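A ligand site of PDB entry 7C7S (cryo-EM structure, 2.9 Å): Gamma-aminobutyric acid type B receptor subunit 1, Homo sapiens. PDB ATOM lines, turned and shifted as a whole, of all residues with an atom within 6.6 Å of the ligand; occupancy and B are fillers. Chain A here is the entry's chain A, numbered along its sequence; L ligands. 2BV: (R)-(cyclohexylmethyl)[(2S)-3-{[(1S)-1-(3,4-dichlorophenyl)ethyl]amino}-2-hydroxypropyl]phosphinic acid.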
ATOM      1  N   GLY A 183      20.404  30.084  28.207  1.00  0.00           N
ATOM      2  CA  GLY A 183      20.314  30.106  26.757  1.00  0.00           C
ATOM      3  C   GLY A 183      19.650  28.875  26.174  1.00  0.00           C
ATOM      4  O   GLY A 183      19.079  28.945  25.086  1.00  0.00           O
ATOM      5  N   TRP A 184      19.711  27.753  26.866  1.00  0.00           N
ATOM      6  CA  TRP A 184      19.089  26.521  26.401  1.00  0.00           C
ATOM      7  C   TRP A 184      18.616  25.715  27.597  1.00  0.00           C
ATOM      8  O   TRP A 184      19.395  24.972  28.205  1.00  0.00           O
ATOM      9  CB  TRP A 184      20.056  25.699  25.545  1.00  0.00           C
ATOM     10  CG  TRP A 184      19.464  24.419  25.087  1.00  0.00           C
ATOM     11  CD1 TRP A 184      18.381  24.256  24.287  1.00  0.00           C
ATOM     12  CD2 TRP A 184      19.921  23.103  25.424  1.00  0.00           C
ATOM     13  NE1 TRP A 184      18.130  22.931  24.085  1.00  0.00           N
ATOM     14  CE2 TRP A 184      19.063  22.203  24.773  1.00  0.00           C
ATOM     15  CE3 TRP A 184      20.969  22.599  26.190  1.00  0.00           C
ATOM     16  CZ2 TRP A 184      19.222  20.824  24.881  1.00  0.00           C
ATOM     17  CZ3 TRP A 184      21.117  21.242  26.294  1.00  0.00           C
ATOM     18  CH2 TRP A 184      20.252  20.368  25.653  1.00  0.00           C
ATOM     19  N   CYS A 222      23.442  26.993  32.314  1.00  0.00           N
ATOM     20  CA  CYS A 222      24.324  27.244  31.184  1.00  0.00           C
ATOM     21  C   CYS A 222      25.293  28.397  31.446  1.00  0.00           C
ATOM     22  O   CYS A 222      25.761  29.046  30.513  1.00  0.00           O
ATOM     23  CB  CYS A 222      23.533  27.496  29.901  1.00  0.00           C
ATOM     24  SG  CYS A 222      23.022  26.008  29.023  1.00  0.00           S
ATOM     25  N   GLY A 247      25.545  19.338  30.271  1.00  0.00           N
ATOM     26  CA  GLY A 247      24.574  19.630  29.237  1.00  0.00           C
ATOM     27  C   GLY A 247      25.107  20.491  28.111  1.00  0.00           C
ATOM     28  O   GLY A 247      25.799  19.996  27.213  1.00  0.00           O
ATOM     29  N   CYS A 248      24.794  21.787  28.136  1.00  0.00           N
ATOM     30  CA  CYS A 248      25.126  22.695  27.059  1.00  0.00           C
ATOM     31  C   CYS A 248      26.642  22.857  26.909  1.00  0.00           C
ATOM     32  O   CYS A 248      27.432  22.309  27.672  1.00  0.00           O
ATOM     33  CB  CYS A 248      24.446  24.040  27.269  1.00  0.00           C
ATOM     34  SG  CYS A 248      24.699  24.870  28.839  1.00  0.00           S
ATOM     35  N   SER A 249      27.027  23.611  25.884  1.00  0.00           N
ATOM     36  CA  SER A 249      28.354  23.486  25.294  1.00  0.00           C
ATOM     37  C   SER A 249      29.439  24.202  26.084  1.00  0.00           C
ATOM     38  O   SER A 249      30.570  23.724  26.155  1.00  0.00           O
ATOM     39  CB  SER A 249      28.313  23.983  23.852  1.00  0.00           C
ATOM     40  OG  SER A 249      29.575  23.844  23.265  1.00  0.00           O
ATOM     41  N   SER A 250      29.134  25.370  26.654  1.00  0.00           N
ATOM     42  CA  SER A 250      30.155  26.099  27.427  1.00  0.00           C
ATOM     43  C   SER A 250      30.512  25.349  28.706  1.00  0.00           C
ATOM     44  O   SER A 250      31.697  25.187  29.038  1.00  0.00           O
ATOM     45  CB  SER A 250      29.643  27.498  27.749  1.00  0.00           C
ATOM     46  OG  SER A 250      28.386  27.422  28.385  1.00  0.00           O
ATOM     47  N   SER A 252      30.162  22.239  29.017  1.00  0.00           N
ATOM     48  CA  SER A 252      30.833  21.024  28.585  1.00  0.00           C
ATOM     49  C   SER A 252      32.295  21.288  28.292  1.00  0.00           C
ATOM     50  O   SER A 252      33.143  20.441  28.590  1.00  0.00           O
ATOM     51  CB  SER A 252      30.125  20.445  27.361  1.00  0.00           C
ATOM     52  OG  SER A 252      28.728  20.458  27.577  1.00  0.00           O
ATOM     53  N   GLY A 270      24.079  17.167  25.233  1.00  0.00           N
ATOM     54  CA  GLY A 270      23.452  18.275  24.550  1.00  0.00           C
ATOM     55  C   GLY A 270      24.365  19.319  23.953  1.00  0.00           C
ATOM     56  O   GLY A 270      23.904  20.425  23.667  1.00  0.00           O
ATOM     57  N   SER A 271      25.640  19.020  23.753  1.00  0.00           N
ATOM     58  CA  SER A 271      26.599  20.012  23.266  1.00  0.00           C
ATOM     59  C   SER A 271      26.910  19.787  21.804  1.00  0.00           C
ATOM     60  O   SER A 271      27.288  18.683  21.410  1.00  0.00           O
ATOM     61  CB  SER A 271      27.889  19.970  24.081  1.00  0.00           C
ATOM     62  OG  SER A 271      28.614  18.788  23.808  1.00  0.00           O
ATOM     63  N   SER A 272      26.808  20.853  21.002  1.00  0.00           N
ATOM     64  CA  SER A 272      26.946  20.767  19.559  1.00  0.00           C
ATOM     65  C   SER A 272      28.150  21.530  19.016  1.00  0.00           C
ATOM     66  O   SER A 272      28.270  21.683  17.797  1.00  0.00           O
ATOM     67  CB  SER A 272      25.678  21.282  18.879  1.00  0.00           C
ATOM     68  OG  SER A 272      25.532  22.665  19.075  1.00  0.00           O
ATOM     69  N   SER A 273      29.034  21.998  19.869  1.00  0.00           N
ATOM     70  CA  SER A 273      30.143  22.825  19.415  1.00  0.00           C
ATOM     71  C   SER A 273      31.157  21.993  18.663  1.00  0.00           C
ATOM     72  O   SER A 273      31.528  20.912  19.121  1.00  0.00           O
ATOM     73  CB  SER A 273      30.814  23.504  20.598  1.00  0.00           C
ATOM     74  OG  SER A 273      31.960  24.232  20.184  1.00  0.00           O
ATOM     75  N   LEU A 276      34.588  21.061  20.659  1.00  0.00           N
ATOM     76  CA  LEU A 276      34.672  19.915  21.555  1.00  0.00           C
ATOM     77  C   LEU A 276      35.144  18.651  20.852  1.00  0.00           C
ATOM     78  O   LEU A 276      35.302  17.637  21.522  1.00  0.00           O
ATOM     79  CB  LEU A 276      33.326  19.684  22.217  1.00  0.00           C
ATOM     80  CG  LEU A 276      32.998  20.624  23.381  1.00  0.00           C
ATOM     81  CD1 LEU A 276      31.512  20.659  23.635  1.00  0.00           C
ATOM     82  CD2 LEU A 276      33.739  20.176  24.601  1.00  0.00           C
ATOM     83  N   ARG A 287      30.041  12.368  23.425  1.00  0.00           N
ATOM     84  CA  ARG A 287      28.733  13.013  23.395  1.00  0.00           C
ATOM     85  C   ARG A 287      27.817  12.267  22.445  1.00  0.00           C
ATOM     86  O   ARG A 287      28.239  11.787  21.403  1.00  0.00           O
ATOM     87  CB  ARG A 287      28.834  14.477  22.962  1.00  0.00           C
ATOM     88  CG  ARG A 287      29.655  14.714  21.737  1.00  0.00           C
ATOM     89  CD  ARG A 287      29.469  16.128  21.272  1.00  0.00           C
ATOM     90  NE  ARG A 287      30.558  16.594  20.432  1.00  0.00           N
ATOM     91  CZ  ARG A 287      30.616  17.832  19.959  1.00  0.00           C
ATOM     92  NH1 ARG A 287      29.651  18.683  20.251  1.00  0.00           N
ATOM     93  NH2 ARG A 287      31.632  18.204  19.207  1.00  0.00           N
ATOM     94  N   HIS A 289      25.130  13.973  21.378  1.00  0.00           N
ATOM     95  CA  HIS A 289      24.718  15.054  20.501  1.00  0.00           C
ATOM     96  C   HIS A 289      25.777  15.259  19.440  1.00  0.00           C
ATOM     97  O   HIS A 289      26.942  15.457  19.783  1.00  0.00           O
ATOM     98  CB  HIS A 289      24.524  16.323  21.303  1.00  0.00           C
ATOM     99  CG  HIS A 289      23.736  17.380  20.588  1.00  0.00           C
ATOM    100  ND1 HIS A 289      24.139  17.927  19.398  1.00  0.00           N
ATOM    101  CD2 HIS A 289      22.570  17.986  20.912  1.00  0.00           C
ATOM    102  CE1 HIS A 289      23.256  18.824  19.004  1.00  0.00           C
ATOM    103  NE2 HIS A 289      22.294  18.880  19.912  1.00  0.00           N
ATOM    104  N   PRO A 290      25.443  15.184  18.155  1.00  0.00           N
ATOM    105  CA  PRO A 290      26.461  15.336  17.118  1.00  0.00           C
ATOM    106  C   PRO A 290      27.004  16.754  17.061  1.00  0.00           C
ATOM    107  O   PRO A 290      26.346  17.721  17.452  1.00  0.00           O
ATOM    108  CB  PRO A 290      25.731  14.965  15.826  1.00  0.00           C
ATOM    109  CG  PRO A 290      24.436  14.357  16.264  1.00  0.00           C
ATOM    110  CD  PRO A 290      24.112  14.950  17.575  1.00  0.00           C
ATOM    111  N   VAL A 320      30.790  29.234  17.124  1.00  0.00           N
ATOM    112  CA  VAL A 320      30.274  27.974  16.590  1.00  0.00           C
ATOM    113  C   VAL A 320      30.099  28.055  15.083  1.00  0.00           C
ATOM    114  O   VAL A 320      30.456  27.133  14.343  1.00  0.00           O
ATOM    115  CB  VAL A 320      28.974  27.577  17.310  1.00  0.00           C
ATOM    116  CG1 VAL A 320      27.922  28.651  17.163  1.00  0.00           C
ATOM    117  CG2 VAL A 320      28.443  26.274  16.754  1.00  0.00           C
ATOM    118  N   TYR A 369      21.290  32.685  13.919  1.00  0.00           N
ATOM    119  CA  TYR A 369      20.186  32.327  14.793  1.00  0.00           C
ATOM    120  C   TYR A 369      18.875  32.928  14.265  1.00  0.00           C
ATOM    121  O   TYR A 369      18.856  33.681  13.296  1.00  0.00           O
ATOM    122  CB  TYR A 369      20.445  32.791  16.214  1.00  0.00           C
ATOM    123  CG  TYR A 369      21.541  32.003  16.896  1.00  0.00           C
ATOM    124  CD1 TYR A 369      21.350  30.691  17.278  1.00  0.00           C
ATOM    125  CD2 TYR A 369      22.781  32.576  17.142  1.00  0.00           C
ATOM    126  CE1 TYR A 369      22.342  29.973  17.882  1.00  0.00           C
ATOM    127  CE2 TYR A 369      23.786  31.861  17.750  1.00  0.00           C
ATOM    128  CZ  TYR A 369      23.562  30.552  18.116  1.00  0.00           C
ATOM    129  OH  TYR A 369      24.554  29.834  18.720  1.00  0.00           O
ATOM    130  N   TRP A 397      16.788  23.919  12.832  1.00  0.00           N
ATOM    131  CA  TRP A 397      16.188  23.886  14.168  1.00  0.00           C
ATOM    132  C   TRP A 397      15.541  25.205  14.573  1.00  0.00           C
ATOM    133  O   TRP A 397      15.436  25.474  15.771  1.00  0.00           O
ATOM    134  CB  TRP A 397      17.209  23.441  15.210  1.00  0.00           C
ATOM    135  CG  TRP A 397      18.570  24.007  15.076  1.00  0.00           C
ATOM    136  CD1 TRP A 397      19.690  23.353  14.656  1.00  0.00           C
ATOM    137  CD2 TRP A 397      18.991  25.328  15.419  1.00  0.00           C
ATOM    138  NE1 TRP A 397      20.767  24.188  14.687  1.00  0.00           N
ATOM    139  CE2 TRP A 397      20.371  25.412  15.143  1.00  0.00           C
ATOM    140  CE3 TRP A 397      18.330  26.455  15.903  1.00  0.00           C
ATOM    141  CZ2 TRP A 397      21.098  26.577  15.353  1.00  0.00           C
ATOM    142  CZ3 TRP A 397      19.054  27.616  16.100  1.00  0.00           C
ATOM    143  CH2 TRP A 397      20.424  27.664  15.828  1.00  0.00           C
ATOM    144  N   TYR A 398      15.095  26.019  13.627  1.00  0.00           N
ATOM    145  CA  TYR A 398      14.243  27.132  14.002  1.00  0.00           C
ATOM    146  C   TYR A 398      12.824  26.613  14.234  1.00  0.00           C
ATOM    147  O   TYR A 398      12.485  25.492  13.884  1.00  0.00           O
ATOM    148  CB  TYR A 398      14.199  28.210  12.927  1.00  0.00           C
ATOM    149  CG  TYR A 398      15.515  28.747  12.406  1.00  0.00           C
ATOM    150  CD1 TYR A 398      16.707  28.573  13.101  1.00  0.00           C
ATOM    151  CD2 TYR A 398      15.558  29.455  11.218  1.00  0.00           C
ATOM    152  CE1 TYR A 398      17.888  29.076  12.605  1.00  0.00           C
ATOM    153  CE2 TYR A 398      16.729  29.958  10.732  1.00  0.00           C
ATOM    154  CZ  TYR A 398      17.888  29.768  11.424  1.00  0.00           C
ATOM    155  OH  TYR A 398      19.057  30.272  10.915  1.00  0.00           O
ATOM    156  N   ILE A 429      19.474  17.530  12.237  1.00  0.00           N
ATOM    157  CA  ILE A 429      19.849  16.213  12.736  1.00  0.00           C
ATOM    158  C   ILE A 429      18.594  15.493  13.188  1.00  0.00           C
ATOM    159  O   ILE A 429      17.701  16.075  13.808  1.00  0.00           O
ATOM    160  CB  ILE A 429      20.859  16.327  13.890  1.00  0.00           C
ATOM    161  CG1 ILE A 429      22.078  17.142  13.450  1.00  0.00           C
ATOM    162  CG2 ILE A 429      21.314  14.957  14.325  1.00  0.00           C
ATOM    163  CD1 ILE A 429      22.969  16.424  12.470  1.00  0.00           C
ATOM    164  N   MET A 431      16.843  13.425  15.591  1.00  0.00           N
ATOM    165  CA  MET A 431      17.022  13.048  16.990  1.00  0.00           C
ATOM    166  C   MET A 431      16.253  11.785  17.327  1.00  0.00           C
ATOM    167  O   MET A 431      16.761  10.924  18.054  1.00  0.00           O
ATOM    168  CB  MET A 431      16.561  14.186  17.905  1.00  0.00           C
ATOM    169  CG  MET A 431      17.205  15.524  17.644  1.00  0.00           C
ATOM    170  SD  MET A 431      18.973  15.559  17.996  1.00  0.00           S
ATOM    171  CE  MET A 431      19.242  17.323  18.074  1.00  0.00           C
ATOM    172  N   GLY A 465      14.223  21.644  25.678  1.00  0.00           N
ATOM    173  CA  GLY A 465      14.979  20.412  25.599  1.00  0.00           C
ATOM    174  C   GLY A 465      14.181  19.182  25.258  1.00  0.00           C
ATOM    175  O   GLY A 465      14.679  18.073  25.439  1.00  0.00           O
ATOM    176  N   GLU A 468      15.667  16.945  22.519  1.00  0.00           N
ATOM    177  CA  GLU A 468      16.945  16.333  22.825  1.00  0.00           C
ATOM    178  C   GLU A 468      16.863  15.224  23.862  1.00  0.00           C
ATOM    179  O   GLU A 468      17.881  14.573  24.112  1.00  0.00           O
ATOM    180  CB  GLU A 468      17.928  17.405  23.332  1.00  0.00           C
ATOM    181  CG  GLU A 468      18.742  18.065  22.248  1.00  0.00           C
ATOM    182  CD  GLU A 468      18.057  19.277  21.677  1.00  0.00           C
ATOM    183  OE1 GLU A 468      16.988  19.653  22.183  1.00  0.00           O
ATOM    184  OE2 GLU A 468      18.574  19.855  20.699  1.00  0.00           O
ATOM    185  N   LEU A 471      18.506  11.907  23.307  1.00  0.00           N
ATOM    186  CA  LEU A 471      19.952  11.878  23.436  1.00  0.00           C
ATOM    187  C   LEU A 471      20.377  11.637  24.876  1.00  0.00           C
ATOM    188  O   LEU A 471      21.352  10.932  25.128  1.00  0.00           O
ATOM    189  CB  LEU A 471      20.553  13.174  22.904  1.00  0.00           C
ATOM    190  CG  LEU A 471      20.183  13.507  21.471  1.00  0.00           C
ATOM    191  CD1 LEU A 471      20.408  14.963  21.214  1.00  0.00           C
ATOM    192  CD2 LEU A 471      20.979  12.664  20.517  1.00  0.00           C
HETATM  193  O1  2BV L   1      25.730  23.198  22.024  1.00  0.00           O
HETATM  194  P   2BV L   1      24.753  24.064  22.698  1.00  0.00           P
HETATM  195  O2  2BV L   1      25.299  24.318  24.169  1.00  0.00           O
HETATM  196  C12 2BV L   1      24.513  25.635  21.804  1.00  0.00           C
HETATM  197  C13 2BV L   1      23.337  26.475  22.351  1.00  0.00           C
HETATM  198  C18 2BV L   1      23.798  27.594  23.290  1.00  0.00           C
HETATM  199  C17 2BV L   1      23.345  29.033  22.963  1.00  0.00           C
HETATM  200  C16 2BV L   1      21.912  29.171  22.440  1.00  0.00           C
HETATM  201  C15 2BV L   1      21.417  28.006  21.575  1.00  0.00           C
HETATM  202  C14 2BV L   1      22.487  26.988  21.184  1.00  0.00           C
HETATM  203  C11 2BV L   1      23.169  23.178  22.836  1.00  0.00           C
HETATM  204  C10 2BV L   1      22.691  22.631  21.481  1.00  0.00           C
HETATM  205  O3  2BV L   1      23.618  21.689  20.908  1.00  0.00           O
HETATM  206  C9  2BV L   1      21.353  21.919  21.688  1.00  0.00           C
HETATM  207  N   2BV L   1      20.845  21.346  20.438  1.00  0.00           N
HETATM  208  C2  2BV L   1      20.807  22.084  19.170  1.00  0.00           C
HETATM  209  C1  2BV L   1      20.280  21.274  17.989  1.00  0.00           C
HETATM  210  C3  2BV L   1      20.140  23.408  19.240  1.00  0.00           C
HETATM  211  C8  2BV L   1      20.754  24.486  18.591  1.00  0.00           C
HETATM  212  C7  2BV L   1      20.219  25.762  18.621  1.00  0.00           C
HETATM  213  C6  2BV L   1      19.012  25.984  19.277  1.00  0.00           C
HETATM  214 CL1  2BV L   1      18.195  27.585  19.352  1.00  0.00          CL
HETATM  215  C5  2BV L   1      18.359  24.837  19.955  1.00  0.00           C
HETATM  216 CL2  2BV L   1      16.846  25.166  20.833  1.00  0.00          CL
HETATM  217  C4  2BV L   1      18.930  23.581  19.940  1.00  0.00           C
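The backbone NH (N) of Ser 249 lies within hydrogen-bond range of an oxygen (O2) of the ligand (2.5 Å).
OE2 of Glu 468 lies within salt-bridge range of N of the ligand (2.7 Å).
The backbone NH of Ser 272 lies within hydrogen-bond range of an oxygen (O1) of the ligand, at 2.8 Å.
OG of Ser 272 is in hydrogen-bond range of O3 of the ligand, 2.8 Å away.
A ring nitrogen (NE2) of His 289 is in hydrogen-bond range of a nitrogen (N) of the ligand (2.9 Å).
The backbone carbonyl oxygen (O) of Gly 270 sits close to an oxygen (O3) of the ligand (3.0 Å).
SG of Cys 248 forms a disulfide with SG of Cys 222 (2.0 Å).
O of Ser 271 lies within hydrogen-bond range of NH1 of Arg 287, at 2.6 Å.
Merely in contact with the ligand: Cys 248, Trp 397, Ser 271, Trp 184 and Gly 183.
Hydrophobic or aromatic side chains within 4 Å of the ligand: Trp 184, His 289 and Trp 397.
Ten residues have an atom within 4 Å of the ligand: Gly 183, Trp 184, Cys 248, Ser 249, Gly 270, Ser 271, Ser 272, His 289, Trp 397 and Glu 468.
Along chain A the residues within 4 Å of the ligand span positions 183 to 468.
The nearest printed residue that does not touch the ligand is Met 431 (4.1 Å).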
